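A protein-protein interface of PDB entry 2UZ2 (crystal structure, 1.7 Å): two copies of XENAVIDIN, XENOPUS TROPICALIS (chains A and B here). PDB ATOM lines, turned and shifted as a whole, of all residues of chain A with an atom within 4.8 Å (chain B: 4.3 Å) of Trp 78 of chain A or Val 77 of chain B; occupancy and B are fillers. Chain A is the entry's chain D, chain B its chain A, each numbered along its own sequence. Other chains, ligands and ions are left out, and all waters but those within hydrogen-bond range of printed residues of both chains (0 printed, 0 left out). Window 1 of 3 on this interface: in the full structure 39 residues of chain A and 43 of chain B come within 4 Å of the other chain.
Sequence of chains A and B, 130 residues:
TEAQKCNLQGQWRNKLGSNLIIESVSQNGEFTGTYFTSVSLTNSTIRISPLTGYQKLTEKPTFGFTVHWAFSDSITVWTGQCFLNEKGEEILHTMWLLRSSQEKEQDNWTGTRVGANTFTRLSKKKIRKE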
ATOM      1  N   TYR A  35      -7.021  24.684  -2.055  1.00  0.00           N
ATOM      2  CA  TYR A  35      -6.068  24.290  -3.096  1.00  0.00           C
ATOM      3  C   TYR A  35      -5.764  25.517  -3.932  1.00  0.00           C
ATOM      4  O   TYR A  35      -6.674  26.263  -4.371  1.00  0.00           O
ATOM      5  CB  TYR A  35      -6.695  23.206  -3.962  1.00  0.00           C
ATOM      6  CG  TYR A  35      -5.689  22.439  -4.753  1.00  0.00           C
ATOM      7  CD1 TYR A  35      -5.238  21.178  -4.308  1.00  0.00           C
ATOM      8  CD2 TYR A  35      -5.231  22.918  -5.958  1.00  0.00           C
ATOM      9  CE1 TYR A  35      -4.325  20.441  -5.067  1.00  0.00           C
ATOM     10  CE2 TYR A  35      -4.293  22.185  -6.707  1.00  0.00           C
ATOM     11  CZ  TYR A  35      -3.857  20.946  -6.236  1.00  0.00           C
ATOM     12  OH  TYR A  35      -2.930  20.261  -7.026  1.00  0.00           O
ATOM     13  N   PHE A  63      -7.188   8.439   0.827  1.00  0.00           N
ATOM     14  CA  PHE A  63      -8.000   9.658   1.032  1.00  0.00           C
ATOM     15  C   PHE A  63      -8.581  10.072  -0.306  1.00  0.00           C
ATOM     16  O   PHE A  63      -8.151   9.568  -1.360  1.00  0.00           O
ATOM     17  CB  PHE A  63      -7.114  10.802   1.555  1.00  0.00           C
ATOM     18  CG  PHE A  63      -5.913  11.069   0.663  1.00  0.00           C
ATOM     19  CD1 PHE A  63      -6.017  11.903  -0.439  1.00  0.00           C
ATOM     20  CD2 PHE A  63      -4.695  10.468   0.959  1.00  0.00           C
ATOM     21  CE1 PHE A  63      -4.896  12.138  -1.290  1.00  0.00           C
ATOM     22  CE2 PHE A  63      -3.580  10.701   0.146  1.00  0.00           C
ATOM     23  CZ  PHE A  63      -3.680  11.510  -0.977  1.00  0.00           C
ATOM     24  N   GLY A  64      -9.572  10.946  -0.263  1.00  0.00           N
ATOM     25  CA  GLY A  64     -10.057  11.551  -1.508  1.00  0.00           C
ATOM     26  C   GLY A  64     -10.580  12.924  -1.190  1.00  0.00           C
ATOM     27  O   GLY A  64     -10.995  13.179  -0.056  1.00  0.00           O
ATOM     28  N   PHE A  65     -10.591  13.813  -2.182  1.00  0.00           N
ATOM     29  CA  PHE A  65     -11.208  15.128  -1.948  1.00  0.00           C
ATOM     30  C   PHE A  65     -11.643  15.779  -3.237  1.00  0.00           C
ATOM     31  O   PHE A  65     -11.201  15.378  -4.317  1.00  0.00           O
ATOM     32  CB  PHE A  65     -10.272  16.074  -1.157  1.00  0.00           C
ATOM     33  CG  PHE A  65      -8.947  16.363  -1.862  1.00  0.00           C
ATOM     34  CD1 PHE A  65      -8.827  17.454  -2.731  1.00  0.00           C
ATOM     35  CD2 PHE A  65      -7.832  15.584  -1.597  1.00  0.00           C
ATOM     36  CE1 PHE A  65      -7.610  17.736  -3.317  1.00  0.00           C
ATOM     37  CE2 PHE A  65      -6.599  15.843  -2.204  1.00  0.00           C
ATOM     38  CZ  PHE A  65      -6.499  16.936  -3.086  1.00  0.00           C
ATOM     39  N   VAL A  67     -12.155  19.617  -5.196  1.00  0.00           N
ATOM     40  CA  VAL A  67     -11.877  21.047  -5.174  1.00  0.00           C
ATOM     41  C   VAL A  67     -12.957  21.743  -5.967  1.00  0.00           C
ATOM     42  O   VAL A  67     -13.247  21.365  -7.088  1.00  0.00           O
ATOM     43  CB  VAL A  67     -10.485  21.388  -5.737  1.00  0.00           C
ATOM     44  CG1 VAL A  67     -10.303  22.902  -5.832  1.00  0.00           C
ATOM     45  CG2 VAL A  67      -9.403  20.823  -4.810  1.00  0.00           C
ATOM     46  N   TRP A  69     -13.485  24.797  -7.745  1.00  0.00           N
ATOM     47  CA  TRP A  69     -12.678  25.919  -8.257  1.00  0.00           C
ATOM     48  C   TRP A  69     -13.498  27.193  -8.176  1.00  0.00           C
ATOM     49  O   TRP A  69     -14.626  27.242  -8.686  1.00  0.00           O
ATOM     50  CB  TRP A  69     -12.250  25.671  -9.715  1.00  0.00           C
ATOM     51  CG  TRP A  69     -11.435  24.425  -9.840  1.00  0.00           C
ATOM     52  CD1 TRP A  69     -11.822  23.259 -10.436  1.00  0.00           C
ATOM     53  CD2 TRP A  69     -10.108  24.206  -9.332  1.00  0.00           C
ATOM     54  NE1 TRP A  69     -10.811  22.316 -10.340  1.00  0.00           N
ATOM     55  CE2 TRP A  69      -9.751  22.874  -9.655  1.00  0.00           C
ATOM     56  CE3 TRP A  69      -9.190  25.010  -8.626  1.00  0.00           C
ATOM     57  CZ2 TRP A  69      -8.499  22.310  -9.310  1.00  0.00           C
ATOM     58  CZ3 TRP A  69      -7.947  24.445  -8.260  1.00  0.00           C
ATOM     59  CH2 TRP A  69      -7.610  23.117  -8.615  1.00  0.00           C
ATOM     60  N   THR A  76     -12.512  19.340  -9.772  1.00  0.00           N
ATOM     61  CA  THR A  76     -11.507  18.265  -9.832  1.00  0.00           C
ATOM     62  C   THR A  76     -11.600  17.434  -8.568  1.00  0.00           C
ATOM     63  O   THR A  76     -11.812  17.991  -7.479  1.00  0.00           O
ATOM     64  CB  THR A  76     -10.085  18.812  -9.967  1.00  0.00           C
ATOM     65  OG1 THR A  76     -10.028  19.682 -11.107  1.00  0.00           O
ATOM     66  CG2 THR A  76      -9.054  17.665 -10.126  1.00  0.00           C
ATOM     67  N   VAL A  77     -11.456  16.124  -8.740  1.00  0.00           N
ATOM     68  CA  VAL A  77     -11.391  15.191  -7.593  1.00  0.00           C
ATOM     69  C   VAL A  77     -10.048  14.491  -7.627  1.00  0.00           C
ATOM     70  O   VAL A  77      -9.526  14.202  -8.698  1.00  0.00           O
ATOM     71  CB  VAL A  77     -12.562  14.163  -7.564  1.00  0.00           C
ATOM     72  CG1 VAL A  77     -13.935  14.888  -7.295  1.00  0.00           C
ATOM     73  CG2 VAL A  77     -12.648  13.316  -8.873  1.00  0.00           C
ATOM     74  N   TRP A  78      -9.491  14.251  -6.440  1.00  0.00           N
ATOM     75  CA  TRP A  78      -8.249  13.477  -6.294  1.00  0.00           C
ATOM     76  C   TRP A  78      -8.497  12.331  -5.344  1.00  0.00           C
ATOM     77  O   TRP A  78      -9.229  12.468  -4.349  1.00  0.00           O
ATOM     78  CB  TRP A  78      -7.163  14.307  -5.606  1.00  0.00           C
ATOM     79  CG  TRP A  78      -6.448  15.350  -6.433  1.00  0.00           C
ATOM     80  CD1 TRP A  78      -5.166  15.268  -6.906  1.00  0.00           C
ATOM     81  CD2 TRP A  78      -6.902  16.673  -6.745  1.00  0.00           C
ATOM     82  NE1 TRP A  78      -4.791  16.452  -7.497  1.00  0.00           N
ATOM     83  CE2 TRP A  78      -5.844  17.325  -7.425  1.00  0.00           C
ATOM     84  CE3 TRP A  78      -8.110  17.368  -6.530  1.00  0.00           C
ATOM     85  CZ2 TRP A  78      -5.953  18.639  -7.896  1.00  0.00           C
ATOM     86  CZ3 TRP A  78      -8.213  18.678  -6.985  1.00  0.00           C
ATOM     87  CH2 TRP A  78      -7.162  19.299  -7.653  1.00  0.00           C
ATOM     88  N   THR A  79      -7.823  11.219  -5.601  1.00  0.00           N
ATOM     89  CA  THR A  79      -7.767  10.141  -4.596  1.00  0.00           C
ATOM     90  C   THR A  79      -6.377   9.521  -4.575  1.00  0.00           C
ATOM     91  O   THR A  79      -5.690   9.432  -5.615  1.00  0.00           O
ATOM     92  CB  THR A  79      -8.891   9.094  -4.790  1.00  0.00           C
ATOM     93  OG1 THR A  79      -8.904   8.199  -3.681  1.00  0.00           O
ATOM     94  CG2 THR A  79      -8.704   8.241  -6.055  1.00  0.00           C
ATOM     95  N   GLY A  80      -5.933   9.089  -3.403  1.00  0.00           N
ATOM     96  CA  GLY A  80      -4.564   8.617  -3.326  1.00  0.00           C
ATOM     97  C   GLY A  80      -4.282   7.955  -2.022  1.00  0.00           C
ATOM     98  O   GLY A  80      -5.198   7.657  -1.253  1.00  0.00           O
ATOM     99  N   THR A  94      -1.301  10.403  -5.853  1.00  0.00           N
ATOM    100  CA  THR A  94      -2.679  10.676  -6.231  1.00  0.00           C
ATOM    101  C   THR A  94      -2.923  10.521  -7.728  1.00  0.00           C
ATOM    102  O   THR A  94      -2.023  10.634  -8.552  1.00  0.00           O
ATOM    103  CB  THR A  94      -3.120  12.121  -5.881  1.00  0.00           C
ATOM    104  OG1 THR A  94      -2.548  13.061  -6.795  1.00  0.00           O
ATOM    105  CG2 THR A  94      -2.723  12.469  -4.371  1.00  0.00           C
ATOM    106  N   MET A  95      -4.178  10.242  -8.019  1.00  0.00           N
ATOM    107  CA  MET A  95      -4.667  10.447  -9.362  1.00  0.00           C
ATOM    108  C   MET A  95      -5.887  11.323  -9.280  1.00  0.00           C
ATOM    109  O   MET A  95      -6.526  11.438  -8.212  1.00  0.00           O
ATOM    110  CB  MET A  95      -4.960   9.118 -10.000  1.00  0.00           C
ATOM    111  CG  MET A  95      -3.701   8.278 -10.030  1.00  0.00           C
ATOM    112  SD  MET A  95      -3.862   6.958 -11.185  1.00  0.00           S
ATOM    113  CE  MET A  95      -3.617   7.871 -12.719  1.00  0.00           C
ATOM    114  N   TRP A  96      -6.179  12.023 -10.363  1.00  0.00           N
ATOM    115  CA  TRP A  96      -7.252  12.993 -10.353  1.00  0.00           C
ATOM    116  C   TRP A  96      -8.110  12.934 -11.606  1.00  0.00           C
ATOM    117  O   TRP A  96      -7.648  12.442 -12.626  1.00  0.00           O
ATOM    118  CB  TRP A  96      -6.714  14.446 -10.170  1.00  0.00           C
ATOM    119  CG  TRP A  96      -5.581  14.852 -11.094  1.00  0.00           C
ATOM    120  CD1 TRP A  96      -4.256  14.843 -10.805  1.00  0.00           C
ATOM    121  CD2 TRP A  96      -5.695  15.344 -12.428  1.00  0.00           C
ATOM    122  NE1 TRP A  96      -3.509  15.289 -11.883  1.00  0.00           N
ATOM    123  CE2 TRP A  96      -4.370  15.611 -12.895  1.00  0.00           C
ATOM    124  CE3 TRP A  96      -6.771  15.584 -13.288  1.00  0.00           C
ATOM    125  CZ2 TRP A  96      -4.106  16.119 -14.176  1.00  0.00           C
ATOM    126  CZ3 TRP A  96      -6.492  16.082 -14.600  1.00  0.00           C
ATOM    127  CH2 TRP A  96      -5.183  16.353 -15.003  1.00  0.00           C
ATOM    128  N   PHE A 119       2.452  14.549  -4.158  1.00  0.00           N
ATOM    129  CA  PHE A 119       2.622  15.729  -3.299  1.00  0.00           C
ATOM    130  C   PHE A 119       3.664  15.449  -2.232  1.00  0.00           C
ATOM    131  O   PHE A 119       3.706  14.351  -1.704  1.00  0.00           O
ATOM    132  CB  PHE A 119       1.302  16.118  -2.621  1.00  0.00           C
ATOM    133  CG  PHE A 119       0.254  16.628  -3.579  1.00  0.00           C
ATOM    134  CD1 PHE A 119       0.044  17.994  -3.746  1.00  0.00           C
ATOM    135  CD2 PHE A 119      -0.553  15.732  -4.295  1.00  0.00           C
ATOM    136  CE1 PHE A 119      -0.939  18.459  -4.633  1.00  0.00           C
ATOM    137  CE2 PHE A 119      -1.552  16.197  -5.158  1.00  0.00           C
ATOM    138  CZ  PHE A 119      -1.750  17.574  -5.303  1.00  0.00           C
ATOM    139  N   PHE B  65     -17.697  14.426  -5.627  1.00  0.00           N
ATOM    140  CA  PHE B  65     -17.841  14.016  -4.221  1.00  0.00           C
ATOM    141  C   PHE B  65     -16.964  12.818  -3.897  1.00  0.00           C
ATOM    142  O   PHE B  65     -16.502  12.109  -4.817  1.00  0.00           O
ATOM    143  CB  PHE B  65     -19.306  13.744  -3.836  1.00  0.00           C
ATOM    144  CG  PHE B  65     -19.978  12.655  -4.638  1.00  0.00           C
ATOM    145  CD1 PHE B  65     -19.989  11.326  -4.185  1.00  0.00           C
ATOM    146  CD2 PHE B  65     -20.665  12.978  -5.814  1.00  0.00           C
ATOM    147  CE1 PHE B  65     -20.666  10.318  -4.945  1.00  0.00           C
ATOM    148  CE2 PHE B  65     -21.329  11.984  -6.575  1.00  0.00           C
ATOM    149  CZ  PHE B  65     -21.334  10.663  -6.133  1.00  0.00           C
ATOM    150  N   THR B  66     -16.699  12.636  -2.603  1.00  0.00           N
ATOM    151  CA  THR B  66     -15.913  11.518  -2.107  1.00  0.00           C
ATOM    152  C   THR B  66     -16.818  10.655  -1.223  1.00  0.00           C
ATOM    153  O   THR B  66     -17.574  11.213  -0.418  1.00  0.00           O
ATOM    154  CB  THR B  66     -14.760  12.044  -1.227  1.00  0.00           C
ATOM    155  OG1 THR B  66     -13.981  12.975  -1.976  1.00  0.00           O
ATOM    156  CG2 THR B  66     -13.902  10.893  -0.711  1.00  0.00           C
ATOM    157  N   THR B  76     -13.682   6.178  -2.810  1.00  0.00           N
ATOM    158  CA  THR B  76     -14.005   6.489  -4.193  1.00  0.00           C
ATOM    159  C   THR B  76     -14.358   7.966  -4.365  1.00  0.00           C
ATOM    160  O   THR B  76     -14.994   8.568  -3.463  1.00  0.00           O
ATOM    161  CB  THR B  76     -15.183   5.624  -4.697  1.00  0.00           C
ATOM    162  OG1 THR B  76     -14.850   4.243  -4.511  1.00  0.00           O
ATOM    163  CG2 THR B  76     -15.477   5.854  -6.225  1.00  0.00           C
ATOM    164  N   VAL B  77     -13.902   8.545  -5.476  1.00  0.00           N
ATOM    165  CA  VAL B  77     -14.295   9.918  -5.827  1.00  0.00           C
ATOM    166  C   VAL B  77     -15.033   9.848  -7.152  1.00  0.00           C
ATOM    167  O   VAL B  77     -14.665   9.071  -8.067  1.00  0.00           O
ATOM    168  CB  VAL B  77     -13.108  10.909  -5.896  1.00  0.00           C
ATOM    169  CG1 VAL B  77     -12.494  11.083  -4.484  1.00  0.00           C
ATOM    170  CG2 VAL B  77     -12.047  10.393  -6.883  1.00  0.00           C
ATOM    171  N   TRP B  78     -16.048  10.694  -7.294  1.00  0.00           N
ATOM    172  CA  TRP B  78     -16.770  10.795  -8.561  1.00  0.00           C
ATOM    173  C   TRP B  78     -16.747  12.242  -8.984  1.00  0.00           C
ATOM    174  O   TRP B  78     -16.832  13.146  -8.153  1.00  0.00           O
ATOM    175  CB  TRP B  78     -18.256  10.491  -8.342  1.00  0.00           C
ATOM    176  CG  TRP B  78     -18.684   9.051  -8.214  1.00  0.00           C
ATOM    177  CD1 TRP B  78     -19.332   8.286  -9.161  1.00  0.00           C
ATOM    178  CD2 TRP B  78     -18.581   8.248  -7.047  1.00  0.00           C
ATOM    179  NE1 TRP B  78     -19.611   7.038  -8.645  1.00  0.00           N
ATOM    180  CE2 TRP B  78     -19.172   6.995  -7.347  1.00  0.00           C
ATOM    181  CE3 TRP B  78     -18.051   8.466  -5.768  1.00  0.00           C
ATOM    182  CZ2 TRP B  78     -19.254   5.956  -6.408  1.00  0.00           C
ATOM    183  CZ3 TRP B  78     -18.118   7.435  -4.829  1.00  0.00           C
ATOM    184  CH2 TRP B  78     -18.718   6.194  -5.154  1.00  0.00           C
ATOM    185  N   MET B  95     -17.742  10.035 -13.927  1.00  0.00           N
ATOM    186  CA  MET B  95     -16.616   9.121 -13.920  1.00  0.00           C
ATOM    187  C   MET B  95     -16.033   9.080 -12.522  1.00  0.00           C
ATOM    188  O   MET B  95     -16.235  10.006 -11.697  1.00  0.00           O
ATOM    189  CB  MET B  95     -15.588   9.508 -14.970  1.00  0.00           C
ATOM    190  CG  MET B  95     -16.205   9.463 -16.357  1.00  0.00           C
ATOM    191  SD  MET B  95     -14.905   9.516 -17.591  1.00  0.00           S
ATOM    192  CE  MET B  95     -14.431   7.772 -17.547  1.00  0.00           C
ATOM    193  N   TRP B  96     -15.376   7.966 -12.199  1.00  0.00           N
ATOM    194  CA  TRP B  96     -14.934   7.765 -10.827  1.00  0.00           C
ATOM    195  C   TRP B  96     -13.562   7.127 -10.751  1.00  0.00           C
ATOM    196  O   TRP B  96     -13.135   6.486 -11.714  1.00  0.00           O
ATOM    197  CB  TRP B  96     -15.971   6.934 -10.010  1.00  0.00           C
ATOM    198  CG  TRP B  96     -16.424   5.628 -10.611  1.00  0.00           C
ATOM    199  CD1 TRP B  96     -17.607   5.392 -11.252  1.00  0.00           C
ATOM    200  CD2 TRP B  96     -15.738   4.373 -10.575  1.00  0.00           C
ATOM    201  NE1 TRP B  96     -17.690   4.087 -11.656  1.00  0.00           N
ATOM    202  CE2 TRP B  96     -16.565   3.427 -11.233  1.00  0.00           C
ATOM    203  CE3 TRP B  96     -14.502   3.959 -10.063  1.00  0.00           C
ATOM    204  CZ2 TRP B  96     -16.195   2.085 -11.412  1.00  0.00           C
ATOM    205  CZ3 TRP B  96     -14.127   2.593 -10.232  1.00  0.00           C
ATOM    206  CH2 TRP B  96     -14.975   1.684 -10.904  1.00  0.00           C
ATOM    207  N   LEU B  97     -12.880   7.362  -9.638  1.00  0.00           N
ATOM    208  CA  LEU B  97     -11.635   6.669  -9.302  1.00  0.00           C
ATOM    209  C   LEU B  97     -11.864   5.999  -7.967  1.00  0.00           C
ATOM    210  O   LEU B  97     -12.276   6.643  -6.996  1.00  0.00           O
ATOM    211  CB  LEU B  97     -10.489   7.642  -9.121  1.00  0.00           C
ATOM    212  CG  LEU B  97     -10.075   8.440 -10.364  1.00  0.00           C
ATOM    213  CD1 LEU B  97      -9.028   9.481  -9.985  1.00  0.00           C
ATOM    214  CD2 LEU B  97      -9.566   7.467 -11.506  1.00  0.00           C
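The side-chain hydroxyl of Thr 66 of chain B is in hydrogen-bond range of the backbone NH of Phe 65 of chain A, 3.5 Å away.
The backbone carbonyl oxygen (O) of Met 95 of chain A lies within hydrogen-bond range of the backbone NH (N) of Thr 79 of chain A. OG1 of Thr 79 of chain A sits at hydrogen-bond distance from O of Phe 63 of chain A (2.8 Å). N of Phe 65 of chain A is in hydrogen-bond range of O of Trp 78 of chain A, 2.9 Å away. O of Val 77 of chain B is in hydrogen-bond range of N of Leu 97 of chain B, 2.9 Å away. The backbone carbonyl oxygen of Phe 65 of chain B sits at hydrogen-bond distance from the backbone NH of Trp 78 of chain B (2.9 Å).
Among the printed residues, merely in contact across the chains: Val 77 of chain A with Trp 78 of chain B (3.5 Å), Gly 64 of chain A with Thr 66 of chain B (3.5 Å), Trp 78 of chain A with Val 77 of chain B (3.5 Å), Val 77 of chain A with Val 77 of chain B (3.6 Å), Thr 79 of chain A with Leu 97 of chain B (3.6 Å), Met 95 of chain A with Leu 97 of chain B (3.6 Å), Trp 96 of chain A with Leu 97 of chain B (3.8 Å) and Gly 64 of chain A with Val 77 of chain B (3.9 Å).
Printed residues of chain B within 4 Å of Gly 64 of chain A: Thr 66 (3.5 Å) and Val 77 (3.9 Å). Printed residues of chain B within 4 Å of Phe 65 of chain A: Thr 66. Thr 76 of chain A touches none of the printed residues of chain B. Trp 78 of chain A touches just one residue of chain B: Val 77. Phe 65 of chain B touches none of the printed residues of chain A. Printed residues of chain A within 4 Å of Val 77 of chain B: Gly 64 (3.9 Å), Val 77 (3.6 Å) and Trp 78 (3.5 Å). Of the printed residues of chain A, Trp 78 of chain B touches Val 77 (3.5 Å). The nearest printed residue of chain A that does not touch Val 77 of chain B is Thr 79 of chain A (4.004 Å).
Of the 8 printed residues of chain B, 4 touch a printed residue of chain A. Hydrophobic or aromatic side chains of chain B that line the printed part of chain A: Val 77 and Leu 97. Along chain A the printed residues that touch a printed residue of chain B span positions 64 to 96.
Val 77 of chain B touches its own counterpart, Val 77 of chain A. Val 77 of chain A touches Trp 78 of chain B, and with the chains exchanged Trp 78 of chain A touches Val 77 of chain B. Positions printed for both chains: 65, 76, 77, 78, 95 and 96. Of the 9 pairs that touch across the chains among the printed residues, 3 have their exchanged pair printed and touching as well.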
